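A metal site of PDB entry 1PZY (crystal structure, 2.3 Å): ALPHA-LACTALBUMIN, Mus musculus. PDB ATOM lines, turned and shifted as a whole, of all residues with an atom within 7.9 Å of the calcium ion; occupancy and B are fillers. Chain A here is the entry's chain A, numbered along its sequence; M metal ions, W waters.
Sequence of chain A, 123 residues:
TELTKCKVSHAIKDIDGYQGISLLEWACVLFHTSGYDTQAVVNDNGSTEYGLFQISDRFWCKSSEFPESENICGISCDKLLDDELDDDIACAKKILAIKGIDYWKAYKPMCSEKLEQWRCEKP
Water W1 lies within hydrogen-bond range of OD2 of Asp 87 (2.5 Å) and OD2 of Asp 82 (2.7 Å).
The calcium ion is bound by O of Lys 79 (2.2 Å), water W1 (2.3 Å), O of Glu 84 (2.3 Å), OD1 of Asp 87 (2.4 Å), OD2 of Asp 88 (2.5 Å), OD1 of Asp 82 (2.5 Å) and water W2 (2.6 Å).
The calcium ion has seven donor atoms within binding distance.
Of the 16 residues printed, 5 come within 4 Å of the calcium ion.
The side-chain hydroxyl (OG1) of Thr 38 sits close to the backbone carbonyl oxygen (O) of Asp 82, at 3.4 Å.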
ATOM      1  N   THR A  38     -33.569   2.128 -24.983  1.00  0.00           N
ATOM      2  CA  THR A  38     -32.453   1.355 -25.549  1.00  0.00           C
ATOM      3  C   THR A  38     -31.692   2.097 -26.651  1.00  0.00           C
ATOM      4  O   THR A  38     -30.597   1.669 -27.038  1.00  0.00           O
ATOM      5  CB  THR A  38     -32.928  -0.010 -26.116  1.00  0.00           C
ATOM      6  OG1 THR A  38     -33.664   0.188 -27.332  1.00  0.00           O
ATOM      7  CG2 THR A  38     -33.817  -0.729 -25.116  1.00  0.00           C
ATOM      8  N   ILE A  75     -16.517  -3.964 -27.996  1.00  0.00           N
ATOM      9  CA  ILE A  75     -17.746  -3.997 -28.774  1.00  0.00           C
ATOM     10  C   ILE A  75     -17.990  -2.639 -29.404  1.00  0.00           C
ATOM     11  O   ILE A  75     -17.577  -1.603 -28.868  1.00  0.00           O
ATOM     12  CB  ILE A  75     -18.953  -4.355 -27.903  1.00  0.00           C
ATOM     13  CG1 ILE A  75     -20.180  -4.579 -28.779  1.00  0.00           C
ATOM     14  CG2 ILE A  75     -19.233  -3.240 -26.907  1.00  0.00           C
ATOM     15  CD1 ILE A  75     -21.415  -4.987 -28.010  1.00  0.00           C
ATOM     16  N   SER A  76     -18.639  -2.650 -30.561  1.00  0.00           N
ATOM     17  CA  SER A  76     -18.980  -1.410 -31.257  1.00  0.00           C
ATOM     18  C   SER A  76     -20.074  -0.751 -30.438  1.00  0.00           C
ATOM     19  O   SER A  76     -20.945  -1.431 -29.896  1.00  0.00           O
ATOM     20  CB  SER A  76     -19.478  -1.724 -32.668  1.00  0.00           C
ATOM     21  OG  SER A  76     -20.184  -0.630 -33.216  1.00  0.00           O
ATOM     22  N   CYS A  77     -20.049   0.574 -30.322  1.00  0.00           N
ATOM     23  CA  CYS A  77     -21.070   1.237 -29.533  1.00  0.00           C
ATOM     24  C   CYS A  77     -22.467   1.025 -30.135  1.00  0.00           C
ATOM     25  O   CYS A  77     -23.478   1.060 -29.425  1.00  0.00           O
ATOM     26  CB  CYS A  77     -20.755   2.731 -29.399  1.00  0.00           C
ATOM     27  SG  CYS A  77     -19.199   3.147 -28.513  1.00  0.00           S
ATOM     28  N   ASP A  78     -22.509   0.782 -31.448  1.00  0.00           N
ATOM     29  CA  ASP A  78     -23.777   0.562 -32.132  1.00  0.00           C
ATOM     30  C   ASP A  78     -24.520  -0.678 -31.664  1.00  0.00           C
ATOM     31  O   ASP A  78     -25.734  -0.770 -31.822  1.00  0.00           O
ATOM     32  CB  ASP A  78     -23.550   0.495 -33.640  1.00  0.00           C
ATOM     33  CG  ASP A  78     -23.112   1.821 -34.216  1.00  0.00           C
ATOM     34  OD1 ASP A  78     -23.828   2.827 -33.996  1.00  0.00           O
ATOM     35  OD2 ASP A  78     -22.061   1.860 -34.898  1.00  0.00           O
ATOM     36  N   LYS A  79     -23.796  -1.631 -31.080  1.00  0.00           N
ATOM     37  CA  LYS A  79     -24.422  -2.838 -30.583  1.00  0.00           C
ATOM     38  C   LYS A  79     -25.124  -2.544 -29.261  1.00  0.00           C
ATOM     39  O   LYS A  79     -25.809  -3.393 -28.707  1.00  0.00           O
ATOM     40  CB  LYS A  79     -23.381  -3.943 -30.383  1.00  0.00           C
ATOM     41  CG  LYS A  79     -22.833  -4.556 -31.669  1.00  0.00           C
ATOM     42  CD  LYS A  79     -23.947  -5.107 -32.547  1.00  0.00           C
ATOM     43  CE  LYS A  79     -23.405  -5.585 -33.886  1.00  0.00           C
ATOM     44  NZ  LYS A  79     -24.508  -5.951 -34.848  1.00  0.00           N
ATOM     45  N   LEU A  80     -24.948  -1.321 -28.755  1.00  0.00           N
ATOM     46  CA  LEU A  80     -25.584  -0.932 -27.499  1.00  0.00           C
ATOM     47  C   LEU A  80     -26.833  -0.104 -27.794  1.00  0.00           C
ATOM     48  O   LEU A  80     -27.426   0.472 -26.893  1.00  0.00           O
ATOM     49  CB  LEU A  80     -24.620  -0.119 -26.640  1.00  0.00           C
ATOM     50  CG  LEU A  80     -23.288  -0.780 -26.281  1.00  0.00           C
ATOM     51  CD1 LEU A  80     -22.389   0.222 -25.560  1.00  0.00           C
ATOM     52  CD2 LEU A  80     -23.538  -2.013 -25.417  1.00  0.00           C
ATOM     53  N   LEU A  81     -27.209  -0.024 -29.069  1.00  0.00           N
ATOM     54  CA  LEU A  81     -28.380   0.751 -29.471  1.00  0.00           C
ATOM     55  C   LEU A  81     -29.534  -0.094 -30.001  1.00  0.00           C
ATOM     56  O   LEU A  81     -30.530   0.456 -30.478  1.00  0.00           O
ATOM     57  CB  LEU A  81     -27.975   1.801 -30.509  1.00  0.00           C
ATOM     58  CG  LEU A  81     -27.067   2.911 -29.968  1.00  0.00           C
ATOM     59  CD1 LEU A  81     -26.535   3.769 -31.116  1.00  0.00           C
ATOM     60  CD2 LEU A  81     -27.843   3.768 -28.975  1.00  0.00           C
ATOM     61  N   ASP A  82     -29.402  -1.419 -29.913  1.00  0.00           N
ATOM     62  CA  ASP A  82     -30.464  -2.316 -30.358  1.00  0.00           C
ATOM     63  C   ASP A  82     -31.311  -2.765 -29.165  1.00  0.00           C
ATOM     64  O   ASP A  82     -31.290  -2.125 -28.123  1.00  0.00           O
ATOM     65  CB  ASP A  82     -29.892  -3.539 -31.096  1.00  0.00           C
ATOM     66  CG  ASP A  82     -28.934  -4.347 -30.235  1.00  0.00           C
ATOM     67  OD1 ASP A  82     -29.211  -4.521 -29.039  1.00  0.00           O
ATOM     68  OD2 ASP A  82     -27.924  -4.821 -30.786  1.00  0.00           O
ATOM     69  N   ASP A  83     -32.065  -3.848 -29.320  1.00  0.00           N
ATOM     70  CA  ASP A  83     -32.919  -4.339 -28.230  1.00  0.00           C
ATOM     71  C   ASP A  83     -32.395  -5.613 -27.592  1.00  0.00           C
ATOM     72  O   ASP A  83     -33.099  -6.265 -26.820  1.00  0.00           O
ATOM     73  CB  ASP A  83     -34.353  -4.567 -28.710  1.00  0.00           C
ATOM     74  CG  ASP A  83     -34.990  -3.313 -29.257  1.00  0.00           C
ATOM     75  OD1 ASP A  83     -34.856  -2.241 -28.633  1.00  0.00           O
ATOM     76  OD2 ASP A  83     -35.641  -3.395 -30.321  1.00  0.00           O
ATOM     77  N   GLU A  84     -31.163  -5.992 -27.929  1.00  0.00           N
ATOM     78  CA  GLU A  84     -30.517  -7.182 -27.379  1.00  0.00           C
ATOM     79  C   GLU A  84     -29.621  -6.685 -26.245  1.00  0.00           C
ATOM     80  O   GLU A  84     -28.486  -6.269 -26.485  1.00  0.00           O
ATOM     81  CB  GLU A  84     -29.646  -7.858 -28.435  1.00  0.00           C
ATOM     82  CG  GLU A  84     -30.255  -7.845 -29.814  1.00  0.00           C
ATOM     83  CD  GLU A  84     -31.431  -8.763 -29.923  1.00  0.00           C
ATOM     84  OE1 GLU A  84     -32.249  -8.806 -28.985  1.00  0.00           O
ATOM     85  OE2 GLU A  84     -31.540  -9.436 -30.975  1.00  0.00           O
ATOM     86  N   LEU A  85     -30.106  -6.749 -25.020  1.00  0.00           N
ATOM     87  CA  LEU A  85     -29.350  -6.251 -23.883  1.00  0.00           C
ATOM     88  C   LEU A  85     -28.243  -7.143 -23.332  1.00  0.00           C
ATOM     89  O   LEU A  85     -27.460  -6.706 -22.486  1.00  0.00           O
ATOM     90  CB  LEU A  85     -30.335  -5.892 -22.776  1.00  0.00           C
ATOM     91  CG  LEU A  85     -31.456  -5.015 -23.336  1.00  0.00           C
ATOM     92  CD1 LEU A  85     -32.309  -4.487 -22.201  1.00  0.00           C
ATOM     93  CD2 LEU A  85     -30.860  -3.850 -24.126  1.00  0.00           C
ATOM     94  N   ASP A  86     -28.129  -8.360 -23.840  1.00  0.00           N
ATOM     95  CA  ASP A  86     -27.109  -9.256 -23.346  1.00  0.00           C
ATOM     96  C   ASP A  86     -25.695  -8.693 -23.464  1.00  0.00           C
ATOM     97  O   ASP A  86     -24.887  -8.872 -22.552  1.00  0.00           O
ATOM     98  CB  ASP A  86     -27.204 -10.623 -24.042  1.00  0.00           C
ATOM     99  CG  ASP A  86     -28.524 -11.345 -23.738  1.00  0.00           C
ATOM    100  OD1 ASP A  86     -28.844 -11.543 -22.547  1.00  0.00           O
ATOM    101  OD2 ASP A  86     -29.249 -11.707 -24.699  1.00  0.00           O
ATOM    102  N   ASP A  87     -25.382  -8.008 -24.560  1.00  0.00           N
ATOM    103  CA  ASP A  87     -24.044  -7.434 -24.679  1.00  0.00           C
ATOM    104  C   ASP A  87     -23.909  -6.115 -23.914  1.00  0.00           C
ATOM    105  O   ASP A  87     -22.802  -5.725 -23.556  1.00  0.00           O
ATOM    106  CB  ASP A  87     -23.597  -7.272 -26.149  1.00  0.00           C
ATOM    107  CG  ASP A  87     -24.625  -6.580 -27.011  1.00  0.00           C
ATOM    108  OD1 ASP A  87     -25.541  -5.939 -26.446  1.00  0.00           O
ATOM    109  OD2 ASP A  87     -24.515  -6.675 -28.250  1.00  0.00           O
ATOM    110  N   ASP A  88     -25.017  -5.432 -23.661  1.00  0.00           N
ATOM    111  CA  ASP A  88     -24.948  -4.201 -22.884  1.00  0.00           C
ATOM    112  C   ASP A  88     -24.713  -4.628 -21.440  1.00  0.00           C
ATOM    113  O   ASP A  88     -23.960  -4.002 -20.700  1.00  0.00           O
ATOM    114  CB  ASP A  88     -26.254  -3.398 -22.949  1.00  0.00           C
ATOM    115  CG  ASP A  88     -26.741  -3.174 -24.373  1.00  0.00           C
ATOM    116  OD1 ASP A  88     -27.105  -2.021 -24.708  1.00  0.00           O
ATOM    117  OD2 ASP A  88     -26.765  -4.148 -25.142  1.00  0.00           O
ATOM    118  N   ILE A  89     -25.374  -5.716 -21.044  1.00  0.00           N
ATOM    119  CA  ILE A  89     -25.227  -6.225 -19.694  1.00  0.00           C
ATOM    120  C   ILE A  89     -23.809  -6.698 -19.419  1.00  0.00           C
ATOM    121  O   ILE A  89     -23.231  -6.392 -18.375  1.00  0.00           O
ATOM    122  CB  ILE A  89     -26.223  -7.356 -19.438  1.00  0.00           C
ATOM    123  CG1 ILE A  89     -27.639  -6.793 -19.403  1.00  0.00           C
ATOM    124  CG2 ILE A  89     -25.889  -8.040 -18.129  1.00  0.00           C
ATOM    125  CD1 ILE A  89     -28.732  -7.849 -19.620  1.00  0.00           C
HETATM  126 CA    CA M   1     -27.237  -4.648 -27.528  1.00  0.00          CA
HETATM  127  O   HOH W   1     -26.903  -6.417 -28.925  1.00  0.00           O
HETATM  128  O   HOH W   2     -28.813  -2.586 -27.092  1.00  0.00           O
